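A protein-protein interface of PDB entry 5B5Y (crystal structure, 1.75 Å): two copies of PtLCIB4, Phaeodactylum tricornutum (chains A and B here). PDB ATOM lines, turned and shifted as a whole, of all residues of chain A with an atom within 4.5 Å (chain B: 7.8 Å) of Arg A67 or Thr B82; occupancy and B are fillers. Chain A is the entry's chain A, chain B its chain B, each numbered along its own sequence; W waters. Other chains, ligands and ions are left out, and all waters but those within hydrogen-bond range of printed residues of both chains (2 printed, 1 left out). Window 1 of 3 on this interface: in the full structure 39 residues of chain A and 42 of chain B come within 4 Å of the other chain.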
ATOM      1  N   CYS A  61      23.393 -27.590   3.294  1.00  0.00           N
ATOM      2  CA  CYS A  61      24.412 -26.748   3.916  1.00  0.00           C
ATOM      3  C   CYS A  61      25.565 -26.430   2.964  1.00  0.00           C
ATOM      4  O   CYS A  61      25.939 -27.237   2.118  1.00  0.00           O
ATOM      5  CB  CYS A  61      24.958 -27.409   5.192  1.00  0.00           C
ATOM      6  SG  CYS A  61      26.147 -26.372   6.096  1.00  0.00           S
ATOM      7  N   SER A  62      26.094 -25.224   3.121  1.00  0.00           N
ATOM      8  CA  SER A  62      27.310 -24.742   2.469  1.00  0.00           C
ATOM      9  C   SER A  62      28.481 -25.707   2.494  1.00  0.00           C
ATOM     10  O   SER A  62      29.291 -25.737   1.568  1.00  0.00           O
ATOM     11  CB  SER A  62      27.748 -23.461   3.159  1.00  0.00           C
ATOM     12  OG  SER A  62      26.661 -22.564   3.254  1.00  0.00           O
ATOM     13  N   ASP A  63      28.582 -26.430   3.604  1.00  0.00           N
ATOM     14  CA  ASP A  63      29.646 -27.396   3.867  1.00  0.00           C
ATOM     15  C   ASP A  63      29.912 -28.289   2.655  1.00  0.00           C
ATOM     16  O   ASP A  63      28.974 -28.840   2.085  1.00  0.00           O
ATOM     17  CB  ASP A  63      29.235 -28.227   5.094  1.00  0.00           C
ATOM     18  CG  ASP A  63      30.372 -29.077   5.654  1.00  0.00           C
ATOM     19  OD1 ASP A  63      31.322 -29.406   4.903  1.00  0.00           O
ATOM     20  OD2 ASP A  63      30.290 -29.420   6.860  1.00  0.00           O
ATOM     21  N   GLU A  64      31.184 -28.420   2.261  1.00  0.00           N
ATOM     22  CA  GLU A  64      31.529 -29.169   1.059  1.00  0.00           C
ATOM     23  C   GLU A  64      31.154 -30.649   1.144  1.00  0.00           C
ATOM     24  O   GLU A  64      30.995 -31.289   0.106  1.00  0.00           O
ATOM     25  CB  GLU A  64      33.028 -29.019   0.737  1.00  0.00           C
ATOM     26  CG  GLU A  64      33.957 -29.777   1.671  1.00  0.00           C
ATOM     27  CD  GLU A  64      34.250 -29.043   2.969  1.00  0.00           C
ATOM     28  OE1 GLU A  64      33.830 -27.873   3.138  1.00  0.00           O
ATOM     29  OE2 GLU A  64      34.900 -29.649   3.840  1.00  0.00           O
ATOM     30  N   VAL A  65      30.954 -31.192   2.354  1.00  0.00           N
ATOM     31  CA  VAL A  65      30.597 -32.610   2.457  1.00  0.00           C
ATOM     32  C   VAL A  65      29.160 -32.920   2.028  1.00  0.00           C
ATOM     33  O   VAL A  65      28.793 -34.082   1.905  1.00  0.00           O
ATOM     34  CB  VAL A  65      30.791 -33.161   3.890  1.00  0.00           C
ATOM     35  CG1 VAL A  65      32.260 -33.062   4.294  1.00  0.00           C
ATOM     36  CG2 VAL A  65      29.885 -32.440   4.865  1.00  0.00           C
ATOM     37  N   THR A  66      28.353 -31.900   1.764  1.00  0.00           N
ATOM     38  CA  THR A  66      26.988 -32.157   1.315  1.00  0.00           C
ATOM     39  C   THR A  66      26.872 -32.245  -0.202  1.00  0.00           C
ATOM     40  O   THR A  66      25.835 -32.661  -0.718  1.00  0.00           O
ATOM     41  CB  THR A  66      25.983 -31.078   1.790  1.00  0.00           C
ATOM     42  OG1 THR A  66      26.283 -29.822   1.172  1.00  0.00           O
ATOM     43  CG2 THR A  66      25.985 -30.932   3.304  1.00  0.00           C
ATOM     44  N   ARG A  67      27.920 -31.865  -0.889  1.00  0.00           N
ATOM     45  CA  ARG A  67      27.927 -31.892  -2.339  1.00  0.00           C
ATOM     46  C   ARG A  67      27.624 -33.248  -3.001  1.00  0.00           C
ATOM     47  O   ARG A  67      27.064 -33.261  -4.056  1.00  0.00           O
ATOM     48  CB  ARG A  67      29.247 -31.346  -2.910  1.00  0.00           C
ATOM     49  CG  ARG A  67      29.676 -29.986  -2.446  1.00  0.00           C
ATOM     50  CD  ARG A  67      28.909 -28.881  -3.064  1.00  0.00           C
ATOM     51  NE  ARG A  67      27.723 -28.592  -2.328  1.00  0.00           N
ATOM     52  CZ  ARG A  67      27.651 -27.810  -1.292  1.00  0.00           C
ATOM     53  NH1 ARG A  67      26.517 -27.585  -0.691  1.00  0.00           N
ATOM     54  NH2 ARG A  67      28.744 -27.290  -0.823  1.00  0.00           N
ATOM     55  N   PRO A  68      27.999 -34.372  -2.386  1.00  0.00           N
ATOM     56  CA  PRO A  68      27.721 -35.644  -3.083  1.00  0.00           C
ATOM     57  C   PRO A  68      26.246 -35.925  -3.363  1.00  0.00           C
ATOM     58  O   PRO A  68      25.932 -36.518  -4.403  1.00  0.00           O
ATOM     59  CB  PRO A  68      28.272 -36.696  -2.120  1.00  0.00           C
ATOM     60  CG  PRO A  68      29.421 -36.008  -1.464  1.00  0.00           C
ATOM     61  CD  PRO A  68      28.971 -34.571  -1.289  1.00  0.00           C
ATOM     62  N   LEU A  69      25.368 -35.503  -2.457  1.00  0.00           N
ATOM     63  CA  LEU A  69      23.939 -35.662  -2.653  1.00  0.00           C
ATOM     64  C   LEU A  69      23.445 -34.880  -3.870  1.00  0.00           C
ATOM     65  O   LEU A  69      22.664 -35.397  -4.661  1.00  0.00           O
ATOM     66  CB  LEU A  69      23.178 -35.218  -1.403  1.00  0.00           C
ATOM     67  CG  LEU A  69      21.677 -35.495  -1.410  1.00  0.00           C
ATOM     68  CD1 LEU A  69      21.395 -36.966  -1.700  1.00  0.00           C
ATOM     69  CD2 LEU A  69      21.068 -35.057  -0.069  1.00  0.00           C
ATOM     70  N   GLU A  70      23.902 -33.638  -4.009  1.00  0.00           N
ATOM     71  CA  GLU A  70      23.562 -32.818  -5.165  1.00  0.00           C
ATOM     72  C   GLU A  70      24.076 -33.450  -6.449  1.00  0.00           C
ATOM     73  O   GLU A  70      23.382 -33.451  -7.466  1.00  0.00           O
ATOM     74  CB  GLU A  70      24.139 -31.411  -5.027  1.00  0.00           C
ATOM     75  CG  GLU A  70      23.554 -30.630  -3.901  1.00  0.00           C
ATOM     76  CD  GLU A  70      24.195 -29.268  -3.739  1.00  0.00           C
ATOM     77  OE1 GLU A  70      25.318 -29.065  -4.261  1.00  0.00           O
ATOM     78  OE2 GLU A  70      23.565 -28.401  -3.094  1.00  0.00           O
ATOM     79  N   GLN A  71      25.293 -33.980  -6.411  1.00  0.00           N
ATOM     80  CA  GLN A  71      25.846 -34.601  -7.609  1.00  0.00           C
ATOM     81  C   GLN A  71      25.043 -35.853  -7.979  1.00  0.00           C
ATOM     82  O   GLN A  71      24.777 -36.092  -9.154  1.00  0.00           O
ATOM     83  CB  GLN A  71      27.325 -34.939  -7.408  1.00  0.00           C
ATOM     84  CG  GLN A  71      27.895 -35.913  -8.430  1.00  0.00           C
ATOM     85  CD  GLN A  71      29.411 -35.975  -8.366  1.00  0.00           C
ATOM     86  OE1 GLN A  71      30.081 -34.943  -8.323  1.00  0.00           O
ATOM     87  NE2 GLN A  71      29.958 -37.185  -8.344  1.00  0.00           N
ATOM     88  N   LEU B  56      38.402 -25.774  -2.534  1.00  0.00           N
ATOM     89  CA  LEU B  56      37.722 -24.830  -3.413  1.00  0.00           C
ATOM     90  C   LEU B  56      36.500 -24.255  -2.701  1.00  0.00           C
ATOM     91  O   LEU B  56      35.729 -24.988  -2.086  1.00  0.00           O
ATOM     92  CB  LEU B  56      37.292 -25.537  -4.699  1.00  0.00           C
ATOM     93  CG  LEU B  56      36.481 -24.754  -5.738  1.00  0.00           C
ATOM     94  CD1 LEU B  56      37.328 -23.663  -6.335  1.00  0.00           C
ATOM     95  CD2 LEU B  56      35.988 -25.697  -6.821  1.00  0.00           C
ATOM     96  N   ALA B  57      36.320 -22.948  -2.782  1.00  0.00           N
ATOM     97  CA  ALA B  57      35.106 -22.341  -2.272  1.00  0.00           C
ATOM     98  C   ALA B  57      34.580 -21.430  -3.385  1.00  0.00           C
ATOM     99  O   ALA B  57      35.370 -20.877  -4.144  1.00  0.00           O
ATOM    100  CB  ALA B  57      35.376 -21.568  -0.992  1.00  0.00           C
ATOM    101  N   THR B  58      33.262 -21.335  -3.522  1.00  0.00           N
ATOM    102  CA  THR B  58      32.691 -20.451  -4.524  1.00  0.00           C
ATOM    103  C   THR B  58      31.650 -19.527  -3.880  1.00  0.00           C
ATOM    104  O   THR B  58      31.043 -19.847  -2.852  1.00  0.00           O
ATOM    105  CB  THR B  58      32.052 -21.238  -5.688  1.00  0.00           C
ATOM    106  OG1 THR B  58      30.805 -21.805  -5.270  1.00  0.00           O
ATOM    107  CG2 THR B  58      32.977 -22.359  -6.151  1.00  0.00           C
ATOM    108  N   SER B  59      31.483 -18.362  -4.486  1.00  0.00           N
ATOM    109  CA  SER B  59      30.372 -17.475  -4.182  1.00  0.00           C
ATOM    110  C   SER B  59      29.818 -17.018  -5.520  1.00  0.00           C
ATOM    111  O   SER B  59      30.260 -16.010  -6.090  1.00  0.00           O
ATOM    112  CB  SER B  59      30.810 -16.289  -3.315  1.00  0.00           C
ATOM    113  OG  SER B  59      29.697 -15.434  -3.038  1.00  0.00           O
ATOM    114  N   LEU B  60      28.872 -17.801  -6.040  1.00  0.00           N
ATOM    115  CA  LEU B  60      28.246 -17.524  -7.331  1.00  0.00           C
ATOM    116  C   LEU B  60      26.728 -17.528  -7.146  1.00  0.00           C
ATOM    117  O   LEU B  60      26.235 -18.026  -6.130  1.00  0.00           O
ATOM    118  CB  LEU B  60      28.667 -18.570  -8.375  1.00  0.00           C
ATOM    119  CG  LEU B  60      30.176 -18.714  -8.638  1.00  0.00           C
ATOM    120  CD1 LEU B  60      30.449 -19.898  -9.569  1.00  0.00           C
ATOM    121  CD2 LEU B  60      30.737 -17.444  -9.241  1.00  0.00           C
ATOM    122  N   ARG B  67      26.219 -23.064 -12.441  1.00  0.00           N
ATOM    123  CA  ARG B  67      26.814 -24.344 -12.040  1.00  0.00           C
ATOM    124  C   ARG B  67      28.018 -24.818 -12.878  1.00  0.00           C
ATOM    125  O   ARG B  67      28.961 -25.375 -12.304  1.00  0.00           O
ATOM    126  CB  ARG B  67      25.756 -25.465 -12.043  1.00  0.00           C
ATOM    127  CG  ARG B  67      24.573 -25.287 -11.078  1.00  0.00           C
ATOM    128  CD  ARG B  67      24.913 -25.430  -9.595  1.00  0.00           C
ATOM    129  NE  ARG B  67      25.397 -24.184  -9.009  1.00  0.00           N
ATOM    130  CZ  ARG B  67      24.627 -23.147  -8.683  1.00  0.00           C
ATOM    131  NH1 ARG B  67      23.318 -23.192  -8.867  1.00  0.00           N
ATOM    132  NH2 ARG B  67      25.166 -22.066  -8.141  1.00  0.00           N
ATOM    133  N   GLU B  70      31.420 -23.903 -11.452  1.00  0.00           N
ATOM    134  CA  GLU B  70      31.738 -24.706 -10.287  1.00  0.00           C
ATOM    135  C   GLU B  70      32.193 -26.103 -10.685  1.00  0.00           C
ATOM    136  O   GLU B  70      33.163 -26.622 -10.131  1.00  0.00           O
ATOM    137  CB  GLU B  70      30.528 -24.809  -9.355  1.00  0.00           C
ATOM    138  CG  GLU B  70      30.124 -23.492  -8.768  1.00  0.00           C
ATOM    139  CD  GLU B  70      28.779 -23.558  -8.065  1.00  0.00           C
ATOM    140  OE1 GLU B  70      28.106 -24.611  -8.150  1.00  0.00           O
ATOM    141  OE2 GLU B  70      28.406 -22.558  -7.424  1.00  0.00           O
ATOM    142  N   GLY B  78      38.178 -30.511  -6.677  1.00  0.00           N
ATOM    143  CA  GLY B  78      37.278 -31.362  -5.916  1.00  0.00           C
ATOM    144  C   GLY B  78      36.016 -30.647  -5.469  1.00  0.00           C
ATOM    145  O   GLY B  78      35.743 -29.531  -5.913  1.00  0.00           O
ATOM    146  N   LYS B  79      35.254 -31.292  -4.585  1.00  0.00           N
ATOM    147  CA  LYS B  79      34.006 -30.738  -4.069  1.00  0.00           C
ATOM    148  C   LYS B  79      34.241 -29.421  -3.334  1.00  0.00           C
ATOM    149  O   LYS B  79      35.177 -29.296  -2.555  1.00  0.00           O
ATOM    150  CB  LYS B  79      33.322 -31.738  -3.126  1.00  0.00           C
ATOM    151  CG  LYS B  79      32.464 -32.805  -3.826  1.00  0.00           C
ATOM    152  CD  LYS B  79      33.267 -33.718  -4.746  1.00  0.00           C
ATOM    153  CE  LYS B  79      32.371 -34.779  -5.396  1.00  0.00           C
ATOM    154  NZ  LYS B  79      33.138 -35.669  -6.314  1.00  0.00           N
ATOM    155  N   HIS B  80      33.360 -28.459  -3.575  1.00  0.00           N
ATOM    156  CA  HIS B  80      33.551 -27.099  -3.103  1.00  0.00           C
ATOM    157  C   HIS B  80      32.609 -26.726  -1.957  1.00  0.00           C
ATOM    158  O   HIS B  80      31.514 -27.290  -1.800  1.00  0.00           O
ATOM    159  CB  HIS B  80      33.339 -26.115  -4.254  1.00  0.00           C
ATOM    160  CG  HIS B  80      31.937 -26.119  -4.781  1.00  0.00           C
ATOM    161  ND1 HIS B  80      31.455 -27.120  -5.596  1.00  0.00           N
ATOM    162  CD2 HIS B  80      30.907 -25.261  -4.590  1.00  0.00           C
ATOM    163  CE1 HIS B  80      30.189 -26.877  -5.887  1.00  0.00           C
ATOM    164  NE2 HIS B  80      29.833 -25.754  -5.292  1.00  0.00           N
ATOM    165  N   PHE B  81      33.059 -25.746  -1.179  1.00  0.00           N
ATOM    166  CA  PHE B  81      32.267 -25.098  -0.152  1.00  0.00           C
ATOM    167  C   PHE B  81      31.517 -23.957  -0.831  1.00  0.00           C
ATOM    168  O   PHE B  81      32.097 -23.261  -1.654  1.00  0.00           O
ATOM    169  CB  PHE B  81      33.195 -24.584   0.953  1.00  0.00           C
ATOM    170  CG  PHE B  81      32.485 -23.985   2.117  1.00  0.00           C
ATOM    171  CD1 PHE B  81      31.985 -22.700   2.052  1.00  0.00           C
ATOM    172  CD2 PHE B  81      32.348 -24.694   3.306  1.00  0.00           C
ATOM    173  CE1 PHE B  81      31.342 -22.136   3.127  1.00  0.00           C
ATOM    174  CE2 PHE B  81      31.706 -24.134   4.386  1.00  0.00           C
ATOM    175  CZ  PHE B  81      31.194 -22.854   4.303  1.00  0.00           C
ATOM    176  N   THR B  82      30.239 -23.779  -0.523  1.00  0.00           N
ATOM    177  CA  THR B  82      29.464 -22.717  -1.182  1.00  0.00           C
ATOM    178  C   THR B  82      29.208 -21.561  -0.227  1.00  0.00           C
ATOM    179  O   THR B  82      28.619 -21.746   0.835  1.00  0.00           O
ATOM    180  CB  THR B  82      28.107 -23.218  -1.718  1.00  0.00           C
ATOM    181  OG1 THR B  82      27.301 -23.676  -0.631  1.00  0.00           O
ATOM    182  CG2 THR B  82      28.299 -24.367  -2.692  1.00  0.00           C
ATOM    183  N   MET B  83      29.630 -20.374  -0.637  1.00  0.00           N
ATOM    184  CA  MET B  83      29.514 -19.161   0.164  1.00  0.00           C
ATOM    185  C   MET B  83      28.423 -18.243  -0.383  1.00  0.00           C
ATOM    186  O   MET B  83      28.097 -17.228   0.236  1.00  0.00           O
ATOM    187  CB  MET B  83      30.846 -18.391   0.167  1.00  0.00           C
ATOM    188  CG  MET B  83      31.940 -18.905   1.082  1.00  0.00           C
ATOM    189  SD  MET B  83      31.695 -18.367   2.791  1.00  0.00           S
ATOM    190  CE  MET B  83      31.745 -16.572   2.634  1.00  0.00           C
ATOM    191  N   GLY B  84      27.881 -18.590  -1.552  1.00  0.00           N
ATOM    192  CA  GLY B  84      27.090 -17.654  -2.339  1.00  0.00           C
ATOM    193  C   GLY B  84      25.626 -17.541  -1.948  1.00  0.00           C
ATOM    194  O   GLY B  84      25.220 -17.860  -0.826  1.00  0.00           O
ATOM    195  N   GLY B  85      24.838 -17.044  -2.885  1.00  0.00           N
ATOM    196  CA  GLY B  85      23.416 -16.839  -2.681  1.00  0.00           C
ATOM    197  C   GLY B  85      22.954 -15.956  -3.813  1.00  0.00           C
ATOM    198  O   GLY B  85      23.614 -15.886  -4.852  1.00  0.00           O
ATOM    199  N   PRO B  90      28.465 -13.137  -1.176  1.00  0.00           N
ATOM    200  CA  PRO B  90      28.973 -14.147  -0.240  1.00  0.00           C
ATOM    201  C   PRO B  90      28.193 -14.139   1.063  1.00  0.00           C
ATOM    202  O   PRO B  90      28.694 -13.769   2.133  1.00  0.00           O
ATOM    203  CB  PRO B  90      30.439 -13.735  -0.043  1.00  0.00           C
ATOM    204  CG  PRO B  90      30.440 -12.265  -0.277  1.00  0.00           C
ATOM    205  CD  PRO B  90      29.456 -12.071  -1.410  1.00  0.00           C
ATOM    206  N   PHE B  91      26.937 -14.550   0.954  1.00  0.00           N
ATOM    207  CA  PHE B  91      26.025 -14.457   2.074  1.00  0.00           C
ATOM    208  C   PHE B  91      26.372 -15.409   3.210  1.00  0.00           C
ATOM    209  O   PHE B  91      25.880 -15.237   4.318  1.00  0.00           O
ATOM    210  CB  PHE B  91      24.595 -14.687   1.595  1.00  0.00           C
ATOM    211  CG  PHE B  91      24.014 -13.497   0.877  1.00  0.00           C
ATOM    212  CD1 PHE B  91      23.951 -12.267   1.514  1.00  0.00           C
ATOM    213  CD2 PHE B  91      23.542 -13.599  -0.419  1.00  0.00           C
ATOM    214  CE1 PHE B  91      23.417 -11.154   0.872  1.00  0.00           C
ATOM    215  CE2 PHE B  91      22.998 -12.490  -1.064  1.00  0.00           C
ATOM    216  CZ  PHE B  91      22.944 -11.269  -0.416  1.00  0.00           C
ATOM    217  N   GLY B  92      27.215 -16.404   2.946  1.00  0.00           N
ATOM    218  CA  GLY B  92      27.684 -17.277   4.014  1.00  0.00           C
ATOM    219  C   GLY B  92      28.424 -16.461   5.067  1.00  0.00           C
ATOM    220  O   GLY B  92      28.444 -16.807   6.254  1.00  0.00           O
ATOM    221  N   GLY B  93      29.023 -15.361   4.621  1.00  0.00           N
ATOM    222  CA  GLY B  93      29.576 -14.356   5.517  1.00  0.00           C
ATOM    223  C   GLY B  93      30.720 -14.866   6.376  1.00  0.00           C
ATOM    224  O   GLY B  93      31.393 -15.845   6.041  1.00  0.00           O
ATOM    225  N   GLY B  96      30.505 -18.493   7.590  1.00  0.00           N
ATOM    226  CA  GLY B  96      30.739 -19.373   6.465  1.00  0.00           C
ATOM    227  C   GLY B  96      32.237 -19.443   6.168  1.00  0.00           C
ATOM    228  O   GLY B  96      32.770 -20.516   5.958  1.00  0.00           O
ATOM    229  N   PHE B  97      32.913 -18.296   6.167  1.00  0.00           N
ATOM    230  CA  PHE B  97      34.353 -18.277   5.866  1.00  0.00           C
ATOM    231  C   PHE B  97      35.156 -19.036   6.926  1.00  0.00           C
ATOM    232  O   PHE B  97      36.108 -19.747   6.602  1.00  0.00           O
ATOM    233  CB  PHE B  97      34.874 -16.847   5.758  1.00  0.00           C
ATOM    234  CG  PHE B  97      36.340 -16.771   5.439  1.00  0.00           C
ATOM    235  CD1 PHE B  97      36.784 -16.956   4.140  1.00  0.00           C
ATOM    236  CD2 PHE B  97      37.269 -16.550   6.438  1.00  0.00           C
ATOM    237  CE1 PHE B  97      38.132 -16.906   3.843  1.00  0.00           C
ATOM    238  CE2 PHE B  97      38.618 -16.497   6.144  1.00  0.00           C
ATOM    239  CZ  PHE B  97      39.049 -16.679   4.852  1.00  0.00           C
ATOM    240  N   MET B 100      34.601 -22.810   6.480  1.00  0.00           N
ATOM    241  CA  MET B 100      35.391 -23.197   5.326  1.00  0.00           C
ATOM    242  C   MET B 100      36.871 -23.305   5.706  1.00  0.00           C
ATOM    243  O   MET B 100      37.525 -24.304   5.393  1.00  0.00           O
ATOM    244  CB  MET B 100      35.170 -22.182   4.191  1.00  0.00           C
ATOM    245  CG  MET B 100      35.843 -22.529   2.874  1.00  0.00           C
ATOM    246  SD  MET B 100      37.608 -22.133   2.846  1.00  0.00           S
ATOM    247  CE  MET B 100      37.573 -20.345   3.020  1.00  0.00           C
ATOM    248  N   LEU B 112      39.144 -19.259  -3.529  1.00  0.00           N
ATOM    249  CA  LEU B 112      37.788 -18.726  -3.612  1.00  0.00           C
ATOM    250  C   LEU B 112      37.534 -18.132  -4.995  1.00  0.00           C
ATOM    251  O   LEU B 112      38.321 -17.315  -5.485  1.00  0.00           O
ATOM    252  CB  LEU B 112      37.577 -17.666  -2.526  1.00  0.00           C
ATOM    253  CG  LEU B 112      36.325 -16.812  -2.650  1.00  0.00           C
ATOM    254  CD1 LEU B 112      35.094 -17.667  -2.433  1.00  0.00           C
ATOM    255  CD2 LEU B 112      36.396 -15.670  -1.651  1.00  0.00           C
HETATM  256  O   HOH W   1      28.347 -20.368   3.428  1.00  0.00           O
HETATM  257  O   HOH W   2      25.949 -19.606   2.555  1.00  0.00           O
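The backbone NH (N) of Thr B82 sits at hydrogen-bond distance from the backbone carbonyl oxygen (O) of Ser A62 (3.0 Å).
The backbone carbonyl oxygen of His B80 lies within hydrogen-bond range of the guanidinium group of Arg A67 (2.9 Å).
NH1 of Arg A67 lies within hydrogen-bond range of O of Cys A61.
O of Ser A62 sits at hydrogen-bond distance from NH2 of Arg A67 (2.9 Å).
The side-chain hydroxyl (OG1) of Thr A66 is in hydrogen-bond range of the backbone carbonyl oxygen (O) of Asp A63, at 3.0 Å.
The guanidinium group (NH1) of Arg A67 lies within hydrogen-bond range of the side-chain hydroxyl (OG1) of Thr A66, 2.9 Å away.
The guanidinium group of Arg A67 lies within salt-bridge range of the side-chain carboxylate of Glu A70 (3.1 Å).
The backbone NH of Phe B81 sits at hydrogen-bond distance from the backbone carbonyl oxygen of Leu B56 (2.9 Å).
Among the printed residues, merely in contact across the chains: Ser A62 with Phe B81 (3.5 Å), Asp A63 with Phe B81 (3.9 Å), Glu A64 with Lys B79 (3.9 Å), Glu A64 with His B80 (3.4 Å), Glu A64 with Phe B81 (3.5 Å), Arg A67 with Lys B79 (3.6 Å), Arg A67 with Thr B82 (3.5 Å) and Gln A71 with Lys B79 (3.7 Å).
Of the printed residues of chain B, Arg A67 touches Lys B79, His B80 and Thr B82.
No residue of chain B comes within 4 Å of Pro A68.
Of the printed residues of chain B, Ser A62 touches Phe B81 (3.5 Å) and Thr B82 (3.0 Å).
Of the printed residues of chain B, Glu A64 touches Lys B79 (3.9 Å), His B80 (3.4 Å) and Phe B81 (3.5 Å).
Printed residues of chain B within 4 Å of Gln A71: Lys B79.
Cys A61 touches none of the printed residues of chain B.
Leu B56 touches none of the printed residues of chain A.
The nearest residue of chain B that does not touch Arg A67 is Phe B81 (4.2 Å).
The nearest printed residue of chain A that does not touch His B80 is Ser A62 (4.3 Å).
Printed residues of chain A that touch a printed residue of chain B: Ser A62, Asp A63, Glu A64, Arg A67 and Gln A71.
Of the 23 printed residues of chain B, 4 touch a printed residue of chain A.
Among the printed residues, no Asp or Glu carboxylate lies within 4 Å of a Lys or Arg side-chain nitrogen of the other chain.
2 positions are printed for both chains.
Water W1 bridges the side-chain hydroxyl of Ser A62 and the backbone carbonyl oxygen of Thr B82.
Water W2 lies within hydrogen-bond range of OG of Ser A62 and N of Gly B92.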
